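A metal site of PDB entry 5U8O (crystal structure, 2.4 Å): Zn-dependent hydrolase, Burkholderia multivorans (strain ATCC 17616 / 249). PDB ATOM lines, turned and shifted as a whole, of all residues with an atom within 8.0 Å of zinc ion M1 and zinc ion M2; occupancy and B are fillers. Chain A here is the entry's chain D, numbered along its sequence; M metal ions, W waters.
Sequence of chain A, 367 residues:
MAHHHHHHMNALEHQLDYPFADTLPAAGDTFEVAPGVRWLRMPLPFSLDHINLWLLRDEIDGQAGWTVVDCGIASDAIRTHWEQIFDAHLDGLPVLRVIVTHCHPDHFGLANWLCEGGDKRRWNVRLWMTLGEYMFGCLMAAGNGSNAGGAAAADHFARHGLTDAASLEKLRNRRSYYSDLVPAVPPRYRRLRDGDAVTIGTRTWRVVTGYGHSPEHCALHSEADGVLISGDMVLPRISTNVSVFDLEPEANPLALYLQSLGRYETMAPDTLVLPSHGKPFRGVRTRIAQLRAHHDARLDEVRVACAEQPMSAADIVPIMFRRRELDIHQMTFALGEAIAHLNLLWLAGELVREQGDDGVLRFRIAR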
ATOM      1  N   LEU A  44      18.836 -23.888 -10.745  1.00  0.00           N
ATOM      2  CA  LEU A  44      19.195 -22.480 -10.638  1.00  0.00           C
ATOM      3  C   LEU A  44      20.601 -22.397 -10.051  1.00  0.00           C
ATOM      4  O   LEU A  44      20.957 -23.198  -9.183  1.00  0.00           O
ATOM      5  CB  LEU A  44      18.219 -21.696  -9.744  1.00  0.00           C
ATOM      6  CG  LEU A  44      16.764 -21.485 -10.170  1.00  0.00           C
ATOM      7  CD1 LEU A  44      16.030 -20.709  -9.104  1.00  0.00           C
ATOM      8  CD2 LEU A  44      16.695 -20.729 -11.451  1.00  0.00           C
ATOM      9  N   LEU A  48      19.586 -20.963  -3.555  1.00  0.00           N
ATOM     10  CA  LEU A  48      18.331 -21.646  -3.883  1.00  0.00           C
ATOM     11  C   LEU A  48      18.529 -22.266  -5.264  1.00  0.00           C
ATOM     12  O   LEU A  48      18.496 -21.575  -6.275  1.00  0.00           O
ATOM     13  CB  LEU A  48      17.183 -20.651  -3.890  1.00  0.00           C
ATOM     14  CG  LEU A  48      15.753 -21.165  -3.811  1.00  0.00           C
ATOM     15  CD1 LEU A  48      15.636 -22.248  -2.750  1.00  0.00           C
ATOM     16  CD2 LEU A  48      14.774 -20.000  -3.530  1.00  0.00           C
ATOM     17  N   HIS A  50      17.012 -24.377  -7.346  1.00  0.00           N
ATOM     18  CA  HIS A  50      15.996 -24.995  -8.179  1.00  0.00           C
ATOM     19  C   HIS A  50      14.751 -24.121  -8.140  1.00  0.00           C
ATOM     20  O   HIS A  50      14.550 -23.327  -7.224  1.00  0.00           O
ATOM     21  CB  HIS A  50      15.639 -26.387  -7.669  1.00  0.00           C
ATOM     22  CG  HIS A  50      14.885 -26.354  -6.375  1.00  0.00           C
ATOM     23  ND1 HIS A  50      15.508 -26.190  -5.164  1.00  0.00           N
ATOM     24  CD2 HIS A  50      13.562 -26.408  -6.116  1.00  0.00           C
ATOM     25  CE1 HIS A  50      14.601 -26.155  -4.202  1.00  0.00           C
ATOM     26  NE2 HIS A  50      13.412 -26.297  -4.761  1.00  0.00           N
ATOM     27  N   ILE A  51      13.906 -24.302  -9.138  1.00  0.00           N
ATOM     28  CA  ILE A  51      12.545 -23.801  -9.102  1.00  0.00           C
ATOM     29  C   ILE A  51      11.619 -24.856  -9.689  1.00  0.00           C
ATOM     30  O   ILE A  51      12.012 -25.588 -10.606  1.00  0.00           O
ATOM     31  CB  ILE A  51      12.398 -22.456  -9.845  1.00  0.00           C
ATOM     32  CG1 ILE A  51      10.943 -21.979  -9.771  1.00  0.00           C
ATOM     33  CG2 ILE A  51      12.933 -22.591 -11.279  1.00  0.00           C
ATOM     34  CD1 ILE A  51      10.705 -20.553 -10.243  1.00  0.00           C
ATOM     35  N   ASN A  52      10.424 -24.959  -9.127  1.00  0.00           N
ATOM     36  CA  ASN A  52       9.391 -25.839  -9.647  1.00  0.00           C
ATOM     37  C   ASN A  52       8.501 -25.065 -10.605  1.00  0.00           C
ATOM     38  O   ASN A  52       8.013 -23.986 -10.266  1.00  0.00           O
ATOM     39  CB  ASN A  52       8.571 -26.432  -8.517  1.00  0.00           C
ATOM     40  CG  ASN A  52       9.428 -27.163  -7.503  1.00  0.00           C
ATOM     41  OD1 ASN A  52      10.236 -28.042  -7.857  1.00  0.00           O
ATOM     42  ND2 ASN A  52       9.304 -26.785  -6.232  1.00  0.00           N
ATOM     43  N   ASP A  70       4.850 -20.514 -14.816  1.00  0.00           N
ATOM     44  CA  ASP A  70       6.214 -20.058 -14.517  1.00  0.00           C
ATOM     45  C   ASP A  70       7.299 -20.704 -15.392  1.00  0.00           C
ATOM     46  O   ASP A  70       7.091 -21.775 -15.977  1.00  0.00           O
ATOM     47  CB  ASP A  70       6.523 -20.217 -13.020  1.00  0.00           C
ATOM     48  CG  ASP A  70       5.937 -19.077 -12.175  1.00  0.00           C
ATOM     49  OD1 ASP A  70       5.420 -18.098 -12.781  1.00  0.00           O
ATOM     50  OD2 ASP A  70       6.022 -19.132 -10.924  1.00  0.00           O
ATOM     51  N   THR A 101       3.438 -16.225 -12.161  1.00  0.00           N
ATOM     52  CA  THR A 101       2.919 -15.845 -10.857  1.00  0.00           C
ATOM     53  C   THR A 101       3.428 -14.478 -10.428  1.00  0.00           C
ATOM     54  O   THR A 101       2.675 -13.713  -9.807  1.00  0.00           O
ATOM     55  CB  THR A 101       3.283 -16.881  -9.808  1.00  0.00           C
ATOM     56  OG1 THR A 101       4.716 -16.969  -9.702  1.00  0.00           O
ATOM     57  CG2 THR A 101       2.690 -18.256 -10.176  1.00  0.00           C
ATOM     58  N   HIS A 102       4.688 -14.144 -10.715  1.00  0.00           N
ATOM     59  CA  HIS A 102       5.188 -12.823 -10.358  1.00  0.00           C
ATOM     60  C   HIS A 102       6.482 -12.524 -11.125  1.00  0.00           C
ATOM     61  O   HIS A 102       7.042 -13.385 -11.815  1.00  0.00           O
ATOM     62  CB  HIS A 102       5.365 -12.685  -8.833  1.00  0.00           C
ATOM     63  CG  HIS A 102       6.337 -13.638  -8.220  1.00  0.00           C
ATOM     64  ND1 HIS A 102       6.241 -15.003  -8.373  1.00  0.00           N
ATOM     65  CD2 HIS A 102       7.411 -13.418  -7.430  1.00  0.00           C
ATOM     66  CE1 HIS A 102       7.214 -15.594  -7.704  1.00  0.00           C
ATOM     67  NE2 HIS A 102       7.946 -14.659  -7.130  1.00  0.00           N
ATOM     68  N   CYS A 103       6.943 -11.273 -10.998  1.00  0.00           N
ATOM     69  CA  CYS A 103       7.987 -10.715 -11.865  1.00  0.00           C
ATOM     70  C   CYS A 103       9.399 -11.192 -11.529  1.00  0.00           C
ATOM     71  O   CYS A 103      10.331 -10.845 -12.256  1.00  0.00           O
ATOM     72  CB  CYS A 103       7.965  -9.190 -11.793  1.00  0.00           C
ATOM     73  SG  CYS A 103       8.653  -8.585 -10.234  1.00  0.00           S
ATOM     74  N   HIS A 104       9.618 -11.922 -10.459  1.00  0.00           N
ATOM     75  CA  HIS A 104      10.991 -12.216 -10.084  1.00  0.00           C
ATOM     76  C   HIS A 104      11.666 -13.151 -11.098  1.00  0.00           C
ATOM     77  O   HIS A 104      10.996 -13.960 -11.754  1.00  0.00           O
ATOM     78  CB  HIS A 104      11.034 -12.752  -8.663  1.00  0.00           C
ATOM     79  CG  HIS A 104      10.693 -11.700  -7.655  1.00  0.00           C
ATOM     80  ND1 HIS A 104      10.529 -11.966  -6.307  1.00  0.00           N
ATOM     81  CD2 HIS A 104      10.472 -10.368  -7.800  1.00  0.00           C
ATOM     82  CE1 HIS A 104      10.233 -10.841  -5.672  1.00  0.00           C
ATOM     83  NE2 HIS A 104      10.201  -9.862  -6.550  1.00  0.00           N
ATOM     84  N   PRO A 105      12.977 -12.999 -11.301  1.00  0.00           N
ATOM     85  CA  PRO A 105      13.606 -13.550 -12.527  1.00  0.00           C
ATOM     86  C   PRO A 105      13.493 -15.059 -12.702  1.00  0.00           C
ATOM     87  O   PRO A 105      13.479 -15.519 -13.860  1.00  0.00           O
ATOM     88  CB  PRO A 105      15.075 -13.133 -12.376  1.00  0.00           C
ATOM     89  CG  PRO A 105      15.060 -11.993 -11.433  1.00  0.00           C
ATOM     90  CD  PRO A 105      13.922 -12.219 -10.492  1.00  0.00           C
ATOM     91  N   ASP A 106      13.459 -15.858 -11.635  1.00  0.00           N
ATOM     92  CA  ASP A 106      13.364 -17.307 -11.829  1.00  0.00           C
ATOM     93  C   ASP A 106      11.965 -17.739 -12.242  1.00  0.00           C
ATOM     94  O   ASP A 106      11.797 -18.864 -12.711  1.00  0.00           O
ATOM     95  CB  ASP A 106      13.816 -18.049 -10.576  1.00  0.00           C
ATOM     96  CG  ASP A 106      13.237 -17.454  -9.284  1.00  0.00           C
ATOM     97  OD1 ASP A 106      12.943 -18.237  -8.355  1.00  0.00           O
ATOM     98  OD2 ASP A 106      13.073 -16.213  -9.209  1.00  0.00           O
ATOM     99  N   HIS A 107      10.960 -16.875 -12.062  1.00  0.00           N
ATOM    100  CA  HIS A 107       9.611 -17.159 -12.530  1.00  0.00           C
ATOM    101  C   HIS A 107       9.308 -16.572 -13.903  1.00  0.00           C
ATOM    102  O   HIS A 107       8.480 -17.113 -14.638  1.00  0.00           O
ATOM    103  CB  HIS A 107       8.583 -16.647 -11.508  1.00  0.00           C
ATOM    104  CG  HIS A 107       8.779 -17.202 -10.123  1.00  0.00           C
ATOM    105  ND1 HIS A 107       7.974 -18.186  -9.599  1.00  0.00           N
ATOM    106  CD2 HIS A 107       9.691 -16.905  -9.168  1.00  0.00           C
ATOM    107  CE1 HIS A 107       8.385 -18.487  -8.378  1.00  0.00           C
ATOM    108  NE2 HIS A 107       9.426 -17.720  -8.095  1.00  0.00           N
ATOM    109  N   GLU A 133       2.631  -7.172 -11.514  1.00  0.00           N
ATOM    110  CA  GLU A 133       3.851  -7.915 -11.787  1.00  0.00           C
ATOM    111  C   GLU A 133       4.373  -7.622 -13.188  1.00  0.00           C
ATOM    112  O   GLU A 133       5.575  -7.366 -13.372  1.00  0.00           O
ATOM    113  CB  GLU A 133       3.594  -9.419 -11.629  1.00  0.00           C
ATOM    114  CG  GLU A 133       3.105  -9.849 -10.245  1.00  0.00           C
ATOM    115  CD  GLU A 133       4.131  -9.657  -9.144  1.00  0.00           C
ATOM    116  OE1 GLU A 133       5.324  -9.414  -9.444  1.00  0.00           O
ATOM    117  OE2 GLU A 133       3.768  -9.816  -7.961  1.00  0.00           O
ATOM    118  N   HIS A 213       5.498  -9.808  -0.793  1.00  0.00           N
ATOM    119  CA  HIS A 213       6.657 -10.440  -1.404  1.00  0.00           C
ATOM    120  C   HIS A 213       6.990  -9.804  -2.748  1.00  0.00           C
ATOM    121  O   HIS A 213       8.167  -9.664  -3.102  1.00  0.00           O
ATOM    122  CB  HIS A 213       6.426 -11.923  -1.588  1.00  0.00           C
ATOM    123  CG  HIS A 213       7.488 -12.570  -2.398  1.00  0.00           C
ATOM    124  ND1 HIS A 213       8.766 -12.746  -1.929  1.00  0.00           N
ATOM    125  CD2 HIS A 213       7.479 -13.008  -3.676  1.00  0.00           C
ATOM    126  CE1 HIS A 213       9.504 -13.304  -2.870  1.00  0.00           C
ATOM    127  NE2 HIS A 213       8.741 -13.465  -3.937  1.00  0.00           N
ATOM    128  N   SER A 214       5.964  -9.412  -3.490  1.00  0.00           N
ATOM    129  CA  SER A 214       6.099  -8.860  -4.827  1.00  0.00           C
ATOM    130  C   SER A 214       4.878  -7.986  -5.092  1.00  0.00           C
ATOM    131  O   SER A 214       3.942  -7.979  -4.279  1.00  0.00           O
ATOM    132  CB  SER A 214       6.226  -9.988  -5.866  1.00  0.00           C
ATOM    133  OG  SER A 214       5.074 -10.799  -5.886  1.00  0.00           O
ATOM    134  N   HIS A 217       1.317 -10.731  -6.449  1.00  0.00           N
ATOM    135  CA  HIS A 217       1.650 -12.135  -6.680  1.00  0.00           C
ATOM    136  C   HIS A 217       0.382 -12.934  -6.930  1.00  0.00           C
ATOM    137  O   HIS A 217      -0.601 -12.819  -6.198  1.00  0.00           O
ATOM    138  CB  HIS A 217       2.413 -12.633  -5.451  1.00  0.00           C
ATOM    139  CG  HIS A 217       2.848 -14.066  -5.515  1.00  0.00           C
ATOM    140  ND1 HIS A 217       1.989 -15.116  -5.249  1.00  0.00           N
ATOM    141  CD2 HIS A 217       4.045 -14.618  -5.771  1.00  0.00           C
ATOM    142  CE1 HIS A 217       2.642 -16.252  -5.354  1.00  0.00           C
ATOM    143  NE2 HIS A 217       3.891 -15.984  -5.677  1.00  0.00           N
ATOM    144  N   GLY A 231       3.092 -20.394  -5.643  1.00  0.00           N
ATOM    145  CA  GLY A 231       4.171 -19.483  -6.004  1.00  0.00           C
ATOM    146  C   GLY A 231       5.221 -19.378  -4.917  1.00  0.00           C
ATOM    147  O   GLY A 231       5.688 -20.385  -4.353  1.00  0.00           O
ATOM    148  N   ASP A 232       5.585 -18.149  -4.564  1.00  0.00           N
ATOM    149  CA  ASP A 232       6.532 -17.931  -3.487  1.00  0.00           C
ATOM    150  C   ASP A 232       5.871 -17.601  -2.155  1.00  0.00           C
ATOM    151  O   ASP A 232       6.592 -17.414  -1.169  1.00  0.00           O
ATOM    152  CB  ASP A 232       7.482 -16.812  -3.842  1.00  0.00           C
ATOM    153  CG  ASP A 232       8.677 -17.277  -4.626  1.00  0.00           C
ATOM    154  OD1 ASP A 232       8.771 -18.476  -4.941  1.00  0.00           O
ATOM    155  OD2 ASP A 232       9.530 -16.432  -4.910  1.00  0.00           O
ATOM    156  N   MET A 233       4.539 -17.531  -2.092  1.00  0.00           N
ATOM    157  CA  MET A 233       3.903 -17.007  -0.882  1.00  0.00           C
ATOM    158  C   MET A 233       3.913 -18.002   0.276  1.00  0.00           C
ATOM    159  O   MET A 233       3.996 -17.584   1.436  1.00  0.00           O
ATOM    160  CB  MET A 233       2.470 -16.564  -1.182  1.00  0.00           C
ATOM    161  CG  MET A 233       2.326 -15.265  -1.989  1.00  0.00           C
ATOM    162  SD  MET A 233       2.907 -13.759  -1.173  1.00  0.00           S
ATOM    163  CE  MET A 233       1.719 -13.616   0.165  1.00  0.00           C
ATOM    164  N   LEU A 235       6.048 -21.445   1.143  1.00  0.00           N
ATOM    165  CA  LEU A 235       7.094 -22.388   0.814  1.00  0.00           C
ATOM    166  C   LEU A 235       7.347 -23.286   2.025  1.00  0.00           C
ATOM    167  O   LEU A 235       7.460 -22.771   3.152  1.00  0.00           O
ATOM    168  CB  LEU A 235       8.383 -21.644   0.415  1.00  0.00           C
ATOM    169  CG  LEU A 235       8.189 -20.631  -0.724  1.00  0.00           C
ATOM    170  CD1 LEU A 235       9.362 -19.693  -0.895  1.00  0.00           C
ATOM    171  CD2 LEU A 235       7.976 -21.420  -2.019  1.00  0.00           C
ATOM    172  N   ILE A 238      11.428 -22.836   3.470  1.00  0.00           N
ATOM    173  CA  ILE A 238      12.051 -21.538   3.670  1.00  0.00           C
ATOM    174  C   ILE A 238      10.997 -20.461   3.846  1.00  0.00           C
ATOM    175  O   ILE A 238       9.822 -20.634   3.496  1.00  0.00           O
ATOM    176  CB  ILE A 238      13.011 -21.169   2.518  1.00  0.00           C
ATOM    177  CG1 ILE A 238      12.301 -21.312   1.178  1.00  0.00           C
ATOM    178  CG2 ILE A 238      14.254 -22.039   2.584  1.00  0.00           C
ATOM    179  CD1 ILE A 238      13.162 -20.919  -0.005  1.00  0.00           C
ATOM    180  N   THR A 240       9.460 -16.673   3.054  1.00  0.00           N
ATOM    181  CA  THR A 240       9.264 -15.847   1.869  1.00  0.00           C
ATOM    182  C   THR A 240       9.899 -14.485   2.114  1.00  0.00           C
ATOM    183  O   THR A 240       9.636 -13.856   3.143  1.00  0.00           O
ATOM    184  CB  THR A 240       7.763 -15.702   1.589  1.00  0.00           C
ATOM    185  OG1 THR A 240       7.200 -16.997   1.372  1.00  0.00           O
ATOM    186  CG2 THR A 240       7.523 -14.819   0.362  1.00  0.00           C
ATOM    187  N   ASN A 241      10.749 -14.067   1.187  1.00  0.00           N
ATOM    188  CA  ASN A 241      11.484 -12.807   1.321  1.00  0.00           C
ATOM    189  C   ASN A 241      10.538 -11.607   1.253  1.00  0.00           C
ATOM    190  O   ASN A 241       9.702 -11.499   0.354  1.00  0.00           O
ATOM    191  CB  ASN A 241      12.551 -12.720   0.232  1.00  0.00           C
ATOM    192  CG  ASN A 241      13.206 -11.344   0.155  1.00  0.00           C
ATOM    193  OD1 ASN A 241      12.836 -10.511  -0.682  1.00  0.00           O
ATOM    194  ND2 ASN A 241      14.162 -11.104   1.039  1.00  0.00           N
ATOM    195  N   SER A 276       6.773 -23.140  -5.242  1.00  0.00           N
ATOM    196  CA  SER A 276       7.797 -22.890  -6.265  1.00  0.00           C
ATOM    197  C   SER A 276       9.179 -23.397  -5.869  1.00  0.00           C
ATOM    198  O   SER A 276      10.021 -23.597  -6.759  1.00  0.00           O
ATOM    199  CB  SER A 276       7.888 -21.399  -6.589  1.00  0.00           C
ATOM    200  OG  SER A 276       6.729 -20.979  -7.275  1.00  0.00           O
ATOM    201  N   HIS A 277       9.445 -23.591  -4.582  1.00  0.00           N
ATOM    202  CA  HIS A 277      10.685 -24.195  -4.140  1.00  0.00           C
ATOM    203  C   HIS A 277      10.340 -25.169  -3.032  1.00  0.00           C
ATOM    204  O   HIS A 277       9.508 -24.866  -2.171  1.00  0.00           O
ATOM    205  CB  HIS A 277      11.698 -23.156  -3.641  1.00  0.00           C
ATOM    206  CG  HIS A 277      11.796 -21.936  -4.520  1.00  0.00           C
ATOM    207  ND1 HIS A 277      12.572 -21.893  -5.653  1.00  0.00           N
ATOM    208  CD2 HIS A 277      11.231 -20.708  -4.394  1.00  0.00           C
ATOM    209  CE1 HIS A 277      12.480 -20.696  -6.201  1.00  0.00           C
ATOM    210  NE2 HIS A 277      11.671 -19.959  -5.466  1.00  0.00           N
HETATM  211 ZN    ZN M   1      10.008 -14.585  -5.647  1.00  0.00          ZN
HETATM  212 ZN    ZN M   2      11.157 -17.646  -6.329  1.00  0.00          ZN
HETATM  213  O   HOH W   1      12.648 -15.010  -6.607  1.00  0.00           O
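Within 4 Å of zinc ion M2: Asp 106, His 107, Asp 232 and His 277.
Zinc ion M1 is bound by OD2 of Asp 232, 2.0 Å away.
Zinc ion M1 is bound by NE2 of His 213 (2.4 Å).
NE2 of His 102 binds zinc ion M1 (2.5 Å).
Slightly farther from zinc ion M1 lies a ring nitrogen (ND1) of His 104 (2.8 Å).
Slightly farther from zinc ion M1 lies water W1 (2.8 Å).
N of Asp 232 lies within hydrogen-bond range of NE2 of His 217, at 3.0 Å.
The backbone carbonyl oxygen of Asp 232 sits at hydrogen-bond distance from the side-chain hydroxyl of Thr 240 (2.6 Å).
ND1 of His 104 lies close to NE2 of His 213, at 3.3 Å.
A ring nitrogen (ND1) of His 213 sits at hydrogen-bond distance from the backbone carbonyl oxygen of Asn 241 (2.8 Å).
ND1 of His 107 lies within hydrogen-bond range of OD2 of Asp 70.
A ring nitrogen (ND1) of His 107 is in hydrogen-bond range of the side-chain hydroxyl (OG1) of Thr 101 (3.5 Å).
ND1 of His 277 lies within hydrogen-bond range of O of His 50.
The side-chain hydroxyl (OG1) of Thr 101 sits at hydrogen-bond distance from a ring nitrogen (ND1) of His 102 (2.8 Å).
Zinc ion M2 is bound by NE2 of His 107 (2.5 Å), OD2 of Asp 232 (2.5 Å), NE2 of His 277 (2.5 Å) and OD1 of Asp 106 (2.8 Å).
Four residues have an atom within 4 Å of zinc ion M1: His 102, His 104, His 213 and Asp 232.
The nearest printed residue that does not touch zinc ion M1 is His 107 (4.02 Å).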
